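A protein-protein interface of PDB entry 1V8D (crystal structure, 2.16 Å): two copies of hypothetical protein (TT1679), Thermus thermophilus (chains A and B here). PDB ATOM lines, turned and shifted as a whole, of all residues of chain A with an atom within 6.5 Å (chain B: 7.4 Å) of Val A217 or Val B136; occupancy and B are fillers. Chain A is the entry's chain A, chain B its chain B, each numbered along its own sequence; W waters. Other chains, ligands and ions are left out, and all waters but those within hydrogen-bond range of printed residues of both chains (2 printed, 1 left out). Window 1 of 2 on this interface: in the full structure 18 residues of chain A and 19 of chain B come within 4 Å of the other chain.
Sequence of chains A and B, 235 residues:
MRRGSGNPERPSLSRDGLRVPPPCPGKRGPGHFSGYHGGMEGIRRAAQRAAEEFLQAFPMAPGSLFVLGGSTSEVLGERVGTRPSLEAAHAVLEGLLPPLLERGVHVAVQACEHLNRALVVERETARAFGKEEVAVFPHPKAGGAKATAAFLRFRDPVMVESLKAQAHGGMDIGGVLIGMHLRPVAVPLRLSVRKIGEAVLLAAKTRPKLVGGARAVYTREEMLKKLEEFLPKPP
O of Lys A209 lies within hydrogen-bond range of N of Ala B135 (2.8 Å). The backbone NH (N) of Val A211 lies within hydrogen-bond range of the backbone carbonyl oxygen (O) of Ala B135 (3.4 Å). N of Gly A213 lies within hydrogen-bond range of O of His B114 (3.2 Å). N of Ala A214 sits at hydrogen-bond distance from NE2 of His B114, at 3.5 Å. The backbone NH (N) of Arg A215 is in hydrogen-bond range of a ring nitrogen (NE2) of His B114 (3.0 Å). The backbone NH (N) of Phe B137 sits at hydrogen-bond distance from the backbone carbonyl oxygen (O) of Val A217, 3.0 Å away. SD of Met A223 sits close to O of Pro B138.
O of Val A211 sits at hydrogen-bond distance from OH of Tyr A218, at 2.8 Å. The backbone carbonyl oxygen (O) of Gly A212 sits at hydrogen-bond distance from the side-chain hydroxyl (OH) of Tyr A218, at 3.3 Å. The side-chain hydroxyl of Thr A219 is in hydrogen-bond range of the backbone NH of Glu A222, at 2.9 Å. N of Val B134 sits at hydrogen-bond distance from O of Met B159.
Val B134 touches Lys A209. Leu A210 touches Ala B135. Val A211 touches Val B134 (CG2 to CG2, 3.7 Å). CA of Gly A212 touches O of His B114, at 3.2 Å. O of Arg A215 touches CE1 of His B139, at 2.9 Å. Arg A215 touches Ala B142. Ala B142 touches Ala A216 (CB to N, 3.9 Å). CG2 of Val A217 touches ND1 of His B139, at 3.9 Å. O of Ala B135 touches CE2 of Tyr A218, at 3.3 Å. Phe B137 touches Thr A219 (CD2 to N, 3.4 Å).
Printed residues of chain B within 4 Å of Val A217: Val B136, Phe B137 and His B139. Val B136 touches just these residues of chain A: Val A211 (3.2 Å), Ala A216 (3.9 Å), Val A217 (3.5 Å) and Tyr A218 (3.9 Å). Of the printed residues of chain A, Ala B142 touches Arg A215 (3.6 Å) and Ala A216 (3.9 Å). Printed residues of chain B within 4 Å of Ala A214: His B114. Of the printed residues of chain B, Gly A213 touches His B114 (3.2 Å). Val B160 touches none of the printed residues of chain A. The nearest residue of chain A that does not touch Val B136 is Gly A212 (4.9 Å).
Hydrophobic or aromatic side chains of chain B within 4 Å of the printed part of chain A: His B114, Leu B115, Val B134, Ala B135, Val B136, Phe B137, His B139 and Ala B142. Among the printed residues, no Asp or Glu carboxylate lies within 4 Å of a Lys or Arg side-chain nitrogen of the other chain.
No position is printed for both chains.
Water W2 lies within hydrogen-bond range of the backbone carbonyl oxygen of Glu B133 (2.6 Å) and the backbone NH of Lys A209 (3.2 Å). Water W1 lies within hydrogen-bond range of O of Tyr A218 and N of Val B136.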
ATOM      1  N   LYS A 209       5.561 -15.453  -9.592  1.00  0.00           N
ATOM      2  CA  LYS A 209       5.682 -16.766 -10.178  1.00  0.00           C
ATOM      3  C   LYS A 209       6.282 -16.570 -11.561  1.00  0.00           C
ATOM      4  O   LYS A 209       5.859 -15.683 -12.288  1.00  0.00           O
ATOM      5  CB  LYS A 209       4.299 -17.377 -10.395  1.00  0.00           C
ATOM      6  CG  LYS A 209       3.644 -18.025  -9.181  1.00  0.00           C
ATOM      7  CD  LYS A 209       2.249 -18.559  -9.512  1.00  0.00           C
ATOM      8  CE  LYS A 209       1.444 -18.975  -8.217  1.00  0.00           C
ATOM      9  NZ  LYS A 209      -0.010 -19.286  -8.713  1.00  0.00           N
ATOM     10  N   LEU A 210       7.221 -17.447 -11.911  1.00  0.00           N
ATOM     11  CA  LEU A 210       7.868 -17.424 -13.240  1.00  0.00           C
ATOM     12  C   LEU A 210       7.028 -18.251 -14.146  1.00  0.00           C
ATOM     13  O   LEU A 210       6.899 -19.474 -13.912  1.00  0.00           O
ATOM     14  CB  LEU A 210       9.269 -18.055 -13.182  1.00  0.00           C
ATOM     15  CG  LEU A 210      10.241 -17.142 -12.435  1.00  0.00           C
ATOM     16  CD1 LEU A 210      11.349 -18.027 -11.865  1.00  0.00           C
ATOM     17  CD2 LEU A 210      10.764 -16.072 -13.413  1.00  0.00           C
ATOM     18  N   VAL A 211       6.508 -17.651 -15.209  1.00  0.00           N
ATOM     19  CA  VAL A 211       5.575 -18.437 -16.094  1.00  0.00           C
ATOM     20  C   VAL A 211       5.962 -18.425 -17.588  1.00  0.00           C
ATOM     21  O   VAL A 211       6.695 -17.524 -18.028  1.00  0.00           O
ATOM     22  CB  VAL A 211       4.087 -17.828 -16.008  1.00  0.00           C
ATOM     23  CG1 VAL A 211       3.531 -17.884 -14.597  1.00  0.00           C
ATOM     24  CG2 VAL A 211       4.082 -16.405 -16.494  1.00  0.00           C
ATOM     25  N   GLY A 212       5.452 -19.406 -18.347  1.00  0.00           N
ATOM     26  CA  GLY A 212       5.686 -19.443 -19.765  1.00  0.00           C
ATOM     27  C   GLY A 212       6.504 -20.652 -20.084  1.00  0.00           C
ATOM     28  O   GLY A 212       7.318 -21.131 -19.226  1.00  0.00           O
ATOM     29  N   GLY A 213       6.332 -21.144 -21.303  1.00  0.00           N
ATOM     30  CA  GLY A 213       7.059 -22.356 -21.706  1.00  0.00           C
ATOM     31  C   GLY A 213       8.473 -22.067 -22.263  1.00  0.00           C
ATOM     32  O   GLY A 213       9.051 -21.024 -21.988  1.00  0.00           O
ATOM     33  N   ALA A 214       8.970 -22.996 -23.073  1.00  0.00           N
ATOM     34  CA  ALA A 214      10.299 -22.967 -23.636  1.00  0.00           C
ATOM     35  C   ALA A 214      10.773 -21.751 -24.446  1.00  0.00           C
ATOM     36  O   ALA A 214      11.943 -21.445 -24.423  1.00  0.00           O
ATOM     37  CB  ALA A 214      10.514 -24.248 -24.402  1.00  0.00           C
ATOM     38  N   ARG A 215       9.876 -21.056 -25.102  1.00  0.00           N
ATOM     39  CA  ARG A 215      10.193 -19.900 -25.877  1.00  0.00           C
ATOM     40  C   ARG A 215      10.189 -18.616 -25.084  1.00  0.00           C
ATOM     41  O   ARG A 215      10.649 -17.616 -25.565  1.00  0.00           O
ATOM     42  CB  ARG A 215       9.156 -19.751 -26.969  1.00  0.00           C
ATOM     43  CG  ARG A 215       9.300 -20.635 -28.190  1.00  0.00           C
ATOM     44  CD  ARG A 215       8.205 -20.189 -29.157  1.00  0.00           C
ATOM     45  NE  ARG A 215       7.242 -21.270 -29.037  1.00  0.00           N
ATOM     46  CZ  ARG A 215       5.923 -21.177 -28.929  1.00  0.00           C
ATOM     47  NH1 ARG A 215       5.233 -20.026 -28.935  1.00  0.00           N
ATOM     48  NH2 ARG A 215       5.312 -22.307 -28.736  1.00  0.00           N
ATOM     49  N   ALA A 216       9.681 -18.649 -23.860  1.00  0.00           N
ATOM     50  CA  ALA A 216       9.581 -17.415 -23.071  1.00  0.00           C
ATOM     51  C   ALA A 216      10.902 -16.812 -22.615  1.00  0.00           C
ATOM     52  O   ALA A 216      11.867 -17.477 -22.561  1.00  0.00           O
ATOM     53  CB  ALA A 216       8.718 -17.697 -21.810  1.00  0.00           C
ATOM     54  N   VAL A 217      10.909 -15.533 -22.277  1.00  0.00           N
ATOM     55  CA  VAL A 217      12.086 -14.883 -21.720  1.00  0.00           C
ATOM     56  C   VAL A 217      11.679 -14.076 -20.515  1.00  0.00           C
ATOM     57  O   VAL A 217      10.478 -13.724 -20.301  1.00  0.00           O
ATOM     58  CB  VAL A 217      12.836 -14.056 -22.760  1.00  0.00           C
ATOM     59  CG1 VAL A 217      13.238 -15.006 -23.914  1.00  0.00           C
ATOM     60  CG2 VAL A 217      11.995 -12.811 -23.175  1.00  0.00           C
ATOM     61  N   TYR A 218      12.702 -13.803 -19.705  1.00  0.00           N
ATOM     62  CA  TYR A 218      12.522 -13.176 -18.428  1.00  0.00           C
ATOM     63  C   TYR A 218      13.201 -11.898 -18.050  1.00  0.00           C
ATOM     64  O   TYR A 218      13.184 -11.553 -16.870  1.00  0.00           O
ATOM     65  CB  TYR A 218      12.836 -14.236 -17.382  1.00  0.00           C
ATOM     66  CG  TYR A 218      11.943 -15.466 -17.599  1.00  0.00           C
ATOM     67  CD1 TYR A 218      12.322 -16.524 -18.477  1.00  0.00           C
ATOM     68  CD2 TYR A 218      10.653 -15.516 -17.018  1.00  0.00           C
ATOM     69  CE1 TYR A 218      11.410 -17.600 -18.779  1.00  0.00           C
ATOM     70  CE2 TYR A 218       9.765 -16.565 -17.295  1.00  0.00           C
ATOM     71  CZ  TYR A 218      10.142 -17.590 -18.178  1.00  0.00           C
ATOM     72  OH  TYR A 218       9.201 -18.564 -18.508  1.00  0.00           O
ATOM     73  N   THR A 219      13.805 -11.198 -19.024  1.00  0.00           N
ATOM     74  CA  THR A 219      14.458  -9.898 -18.752  1.00  0.00           C
ATOM     75  C   THR A 219      14.094  -8.989 -19.910  1.00  0.00           C
ATOM     76  O   THR A 219      13.820  -9.497 -21.025  1.00  0.00           O
ATOM     77  CB  THR A 219      16.027  -9.996 -18.700  1.00  0.00           C
ATOM     78  OG1 THR A 219      16.506 -10.317 -20.002  1.00  0.00           O
ATOM     79  CG2 THR A 219      16.494 -11.103 -17.706  1.00  0.00           C
ATOM     80  N   GLU A 222      16.520  -9.604 -22.809  1.00  0.00           N
ATOM     81  CA  GLU A 222      16.207 -10.775 -23.677  1.00  0.00           C
ATOM     82  C   GLU A 222      15.046 -10.509 -24.613  1.00  0.00           C
ATOM     83  O   GLU A 222      14.998 -11.029 -25.731  1.00  0.00           O
ATOM     84  CB  GLU A 222      15.866 -12.014 -22.846  1.00  0.00           C
ATOM     85  CG  GLU A 222      17.066 -12.795 -22.424  1.00  0.00           C
ATOM     86  CD  GLU A 222      17.921 -13.149 -23.605  1.00  0.00           C
ATOM     87  OE1 GLU A 222      17.382 -13.673 -24.617  1.00  0.00           O
ATOM     88  OE2 GLU A 222      19.137 -12.890 -23.530  1.00  0.00           O
ATOM     89  N   MET A 223      14.096  -9.724 -24.110  1.00  0.00           N
ATOM     90  CA  MET A 223      12.929  -9.317 -24.856  1.00  0.00           C
ATOM     91  C   MET A 223      13.330  -8.432 -26.047  1.00  0.00           C
ATOM     92  O   MET A 223      12.894  -8.649 -27.172  1.00  0.00           O
ATOM     93  CB  MET A 223      11.978  -8.504 -23.962  1.00  0.00           C
ATOM     94  CG  MET A 223      10.627  -8.282 -24.639  1.00  0.00           C
ATOM     95  SD  MET A 223       9.625  -7.067 -23.846  1.00  0.00           S
ATOM     96  CE  MET A 223      10.775  -5.953 -23.312  1.00  0.00           C
ATOM     97  N   LEU A 224      14.124  -7.398 -25.791  1.00  0.00           N
ATOM     98  CA  LEU A 224      14.506  -6.527 -26.901  1.00  0.00           C
ATOM     99  C   LEU A 224      15.307  -7.313 -27.947  1.00  0.00           C
ATOM    100  O   LEU A 224      15.066  -7.164 -29.098  1.00  0.00           O
ATOM    101  CB  LEU A 224      15.237  -5.297 -26.367  1.00  0.00           C
ATOM    102  CG  LEU A 224      14.524  -4.015 -25.858  1.00  0.00           C
ATOM    103  CD1 LEU A 224      12.973  -4.135 -25.609  1.00  0.00           C
ATOM    104  CD2 LEU A 224      15.300  -3.646 -24.544  1.00  0.00           C
ATOM    105  N   LYS A 226      15.001 -10.512 -28.620  1.00  0.00           N
ATOM    106  CA  LYS A 226      14.014 -11.302 -29.383  1.00  0.00           C
ATOM    107  C   LYS A 226      13.256 -10.406 -30.386  1.00  0.00           C
ATOM    108  O   LYS A 226      12.897 -10.850 -31.486  1.00  0.00           O
ATOM    109  CB  LYS A 226      13.055 -11.967 -28.407  1.00  0.00           C
ATOM    110  CG  LYS A 226      12.971 -13.439 -28.568  1.00  0.00           C
ATOM    111  CD  LYS A 226      14.041 -14.146 -27.904  1.00  0.00           C
ATOM    112  CE  LYS A 226      14.257 -15.438 -28.648  1.00  0.00           C
ATOM    113  NZ  LYS A 226      15.028 -16.425 -27.839  1.00  0.00           N
ATOM    114  N   ALA B 111      -2.081 -12.173 -23.538  1.00  0.00           N
ATOM    115  CA  ALA B 111      -1.039 -12.778 -24.297  1.00  0.00           C
ATOM    116  C   ALA B 111      -1.577 -14.182 -24.638  1.00  0.00           C
ATOM    117  O   ALA B 111      -2.570 -14.641 -24.078  1.00  0.00           O
ATOM    118  CB  ALA B 111       0.286 -12.884 -23.477  1.00  0.00           C
ATOM    119  N   HIS B 114       1.076 -19.667 -24.682  1.00  0.00           N
ATOM    120  CA  HIS B 114       2.456 -20.095 -24.348  1.00  0.00           C
ATOM    121  C   HIS B 114       2.841 -19.326 -23.000  1.00  0.00           C
ATOM    122  O   HIS B 114       3.651 -19.758 -22.213  1.00  0.00           O
ATOM    123  CB  HIS B 114       3.416 -19.764 -25.530  1.00  0.00           C
ATOM    124  CG  HIS B 114       4.786 -20.356 -25.367  1.00  0.00           C
ATOM    125  ND1 HIS B 114       5.061 -21.691 -25.599  1.00  0.00           N
ATOM    126  CD2 HIS B 114       5.949 -19.815 -24.895  1.00  0.00           C
ATOM    127  CE1 HIS B 114       6.325 -21.941 -25.275  1.00  0.00           C
ATOM    128  NE2 HIS B 114       6.884 -20.821 -24.852  1.00  0.00           N
ATOM    129  N   LEU B 115       2.190 -18.205 -22.745  1.00  0.00           N
ATOM    130  CA  LEU B 115       2.442 -17.460 -21.480  1.00  0.00           C
ATOM    131  C   LEU B 115       1.197 -17.595 -20.633  1.00  0.00           C
ATOM    132  O   LEU B 115       0.905 -16.735 -19.810  1.00  0.00           O
ATOM    133  CB  LEU B 115       2.697 -15.944 -21.699  1.00  0.00           C
ATOM    134  CG  LEU B 115       3.811 -15.537 -22.636  1.00  0.00           C
ATOM    135  CD1 LEU B 115       4.067 -14.037 -22.441  1.00  0.00           C
ATOM    136  CD2 LEU B 115       5.000 -16.441 -22.458  1.00  0.00           C
ATOM    137  N   ALA B 118      -1.514 -14.933 -19.622  1.00  0.00           N
ATOM    138  CA  ALA B 118      -1.249 -13.845 -18.669  1.00  0.00           C
ATOM    139  C   ALA B 118      -1.501 -12.562 -19.476  1.00  0.00           C
ATOM    140  O   ALA B 118      -1.325 -12.542 -20.711  1.00  0.00           O
ATOM    141  CB  ALA B 118       0.183 -13.899 -18.147  1.00  0.00           C
ATOM    142  N   GLU B 133       0.711 -10.246 -10.163  1.00  0.00           N
ATOM    143  CA  GLU B 133       1.762 -10.095 -11.157  1.00  0.00           C
ATOM    144  C   GLU B 133       2.550 -11.401 -11.231  1.00  0.00           C
ATOM    145  O   GLU B 133       2.637 -12.155 -10.252  1.00  0.00           O
ATOM    146  CB  GLU B 133       2.673  -8.922 -10.786  1.00  0.00           C
ATOM    147  CG  GLU B 133       3.866  -8.890 -11.782  1.00  0.00           C
ATOM    148  CD  GLU B 133       4.992  -7.818 -11.444  1.00  0.00           C
ATOM    149  OE1 GLU B 133       4.794  -7.012 -10.466  1.00  0.00           O
ATOM    150  OE2 GLU B 133       6.031  -7.816 -12.169  1.00  0.00           O
ATOM    151  N   VAL B 134       2.954 -11.766 -12.438  1.00  0.00           N
ATOM    152  CA  VAL B 134       3.768 -12.965 -12.703  1.00  0.00           C
ATOM    153  C   VAL B 134       4.998 -12.400 -13.426  1.00  0.00           C
ATOM    154  O   VAL B 134       4.945 -11.336 -13.964  1.00  0.00           O
ATOM    155  CB  VAL B 134       2.968 -14.069 -13.586  1.00  0.00           C
ATOM    156  CG1 VAL B 134       1.729 -14.561 -12.770  1.00  0.00           C
ATOM    157  CG2 VAL B 134       2.435 -13.460 -15.021  1.00  0.00           C
ATOM    158  N   ALA B 135       6.041 -13.205 -13.523  1.00  0.00           N
ATOM    159  CA  ALA B 135       7.331 -12.768 -14.055  1.00  0.00           C
ATOM    160  C   ALA B 135       7.581 -13.328 -15.411  1.00  0.00           C
ATOM    161  O   ALA B 135       7.844 -14.534 -15.516  1.00  0.00           O
ATOM    162  CB  ALA B 135       8.525 -13.205 -13.012  1.00  0.00           C
ATOM    163  N   VAL B 136       7.428 -12.474 -16.435  1.00  0.00           N
ATOM    164  CA  VAL B 136       7.701 -12.936 -17.796  1.00  0.00           C
ATOM    165  C   VAL B 136       7.696 -11.698 -18.649  1.00  0.00           C
ATOM    166  O   VAL B 136       7.242 -10.632 -18.231  1.00  0.00           O
ATOM    167  CB  VAL B 136       6.656 -14.032 -18.321  1.00  0.00           C
ATOM    168  CG1 VAL B 136       5.263 -13.407 -18.589  1.00  0.00           C
ATOM    169  CG2 VAL B 136       7.260 -14.794 -19.633  1.00  0.00           C
ATOM    170  N   PHE B 137       8.355 -11.734 -19.784  1.00  0.00           N
ATOM    171  CA  PHE B 137       8.326 -10.533 -20.674  1.00  0.00           C
ATOM    172  C   PHE B 137       7.843 -11.128 -21.945  1.00  0.00           C
ATOM    173  O   PHE B 137       8.355 -12.189 -22.395  1.00  0.00           O
ATOM    174  CB  PHE B 137       9.703  -9.910 -20.865  1.00  0.00           C
ATOM    175  CG  PHE B 137      10.141  -9.045 -19.722  1.00  0.00           C
ATOM    176  CD1 PHE B 137       9.888  -7.685 -19.719  1.00  0.00           C
ATOM    177  CD2 PHE B 137      10.823  -9.568 -18.654  1.00  0.00           C
ATOM    178  CE1 PHE B 137      10.315  -6.878 -18.680  1.00  0.00           C
ATOM    179  CE2 PHE B 137      11.244  -8.734 -17.608  1.00  0.00           C
ATOM    180  CZ  PHE B 137      10.985  -7.394 -17.639  1.00  0.00           C
ATOM    181  N   PRO B 138       6.866 -10.468 -22.575  1.00  0.00           N
ATOM    182  CA  PRO B 138       6.360 -11.040 -23.831  1.00  0.00           C
ATOM    183  C   PRO B 138       7.182 -10.642 -25.076  1.00  0.00           C
ATOM    184  O   PRO B 138       7.805  -9.564 -25.068  1.00  0.00           O
ATOM    185  CB  PRO B 138       4.947 -10.451 -23.943  1.00  0.00           C
ATOM    186  CG  PRO B 138       5.150  -9.072 -23.390  1.00  0.00           C
ATOM    187  CD  PRO B 138       6.103  -9.291 -22.155  1.00  0.00           C
ATOM    188  N   HIS B 139       7.176 -11.500 -26.102  1.00  0.00           N
ATOM    189  CA  HIS B 139       7.803 -11.136 -27.366  1.00  0.00           C
ATOM    190  C   HIS B 139       6.891 -11.812 -28.436  1.00  0.00           C
ATOM    191  O   HIS B 139       6.213 -12.794 -28.130  1.00  0.00           O
ATOM    192  CB  HIS B 139       9.320 -11.478 -27.383  1.00  0.00           C
ATOM    193  CG  HIS B 139       9.632 -12.931 -27.468  1.00  0.00           C
ATOM    194  ND1 HIS B 139       9.894 -13.713 -26.356  1.00  0.00           N
ATOM    195  CD2 HIS B 139       9.739 -13.752 -28.525  1.00  0.00           C
ATOM    196  CE1 HIS B 139      10.159 -14.954 -26.725  1.00  0.00           C
ATOM    197  NE2 HIS B 139      10.075 -14.993 -28.041  1.00  0.00           N
ATOM    198  N   ALA B 142       6.463 -15.635 -28.413  1.00  0.00           N
ATOM    199  CA  ALA B 142       6.044 -16.285 -27.139  1.00  0.00           C
ATOM    200  C   ALA B 142       5.309 -15.201 -26.408  1.00  0.00           C
ATOM    201  O   ALA B 142       5.893 -14.494 -25.572  1.00  0.00           O
ATOM    202  CB  ALA B 142       7.251 -16.730 -26.290  1.00  0.00           C
ATOM    203  N   PHE B 151       2.728  -4.124 -24.276  1.00  0.00           N
ATOM    204  CA  PHE B 151       3.751  -4.053 -23.229  1.00  0.00           C
ATOM    205  C   PHE B 151       4.752  -2.896 -23.559  1.00  0.00           C
ATOM    206  O   PHE B 151       5.142  -2.084 -22.697  1.00  0.00           O
ATOM    207  CB  PHE B 151       4.442  -5.397 -23.092  1.00  0.00           C
ATOM    208  CG  PHE B 151       5.380  -5.476 -21.912  1.00  0.00           C
ATOM    209  CD1 PHE B 151       4.984  -6.077 -20.728  1.00  0.00           C
ATOM    210  CD2 PHE B 151       6.694  -4.907 -21.989  1.00  0.00           C
ATOM    211  CE1 PHE B 151       5.850  -6.140 -19.636  1.00  0.00           C
ATOM    212  CE2 PHE B 151       7.549  -4.964 -20.909  1.00  0.00           C
ATOM    213  CZ  PHE B 151       7.118  -5.595 -19.710  1.00  0.00           C
ATOM    214  N   VAL B 158       2.921  -4.476 -16.425  1.00  0.00           N
ATOM    215  CA  VAL B 158       3.211  -5.690 -15.684  1.00  0.00           C
ATOM    216  C   VAL B 158       2.338  -6.766 -16.328  1.00  0.00           C
ATOM    217  O   VAL B 158       1.309  -6.457 -16.970  1.00  0.00           O
ATOM    218  CB  VAL B 158       2.876  -5.554 -14.169  1.00  0.00           C
ATOM    219  CG1 VAL B 158       3.796  -4.443 -13.522  1.00  0.00           C
ATOM    220  CG2 VAL B 158       1.329  -5.224 -13.980  1.00  0.00           C
ATOM    221  N   MET B 159       2.827  -7.993 -16.244  1.00  0.00           N
ATOM    222  CA  MET B 159       2.146  -9.145 -16.715  1.00  0.00           C
ATOM    223  C   MET B 159       1.345  -9.649 -15.451  1.00  0.00           C
ATOM    224  O   MET B 159       1.893  -9.694 -14.383  1.00  0.00           O
ATOM    225  CB  MET B 159       3.148 -10.206 -17.115  1.00  0.00           C
ATOM    226  CG  MET B 159       4.002  -9.776 -18.295  1.00  0.00           C
ATOM    227  SD  MET B 159       2.930  -9.150 -19.648  1.00  0.00           S
ATOM    228  CE  MET B 159       1.960 -10.690 -20.012  1.00  0.00           C
ATOM    229  N   VAL B 160       0.056  -9.982 -15.601  1.00  0.00           N
ATOM    230  CA  VAL B 160      -0.717 -10.507 -14.455  1.00  0.00           C
ATOM    231  C   VAL B 160      -1.223 -11.920 -14.851  1.00  0.00           C
ATOM    232  O   VAL B 160      -1.400 -12.305 -16.064  1.00  0.00           O
ATOM    233  CB  VAL B 160      -1.939  -9.592 -14.084  1.00  0.00           C
ATOM    234  CG1 VAL B 160      -1.453  -8.268 -13.475  1.00  0.00           C
ATOM    235  CG2 VAL B 160      -2.772  -9.303 -15.344  1.00  0.00           C
HETATM  236  O   HOH W   1      10.710 -11.996 -15.449  1.00  0.00           O
HETATM  237  O   HOH W   2       2.576 -14.402  -8.949  1.00  0.00           O
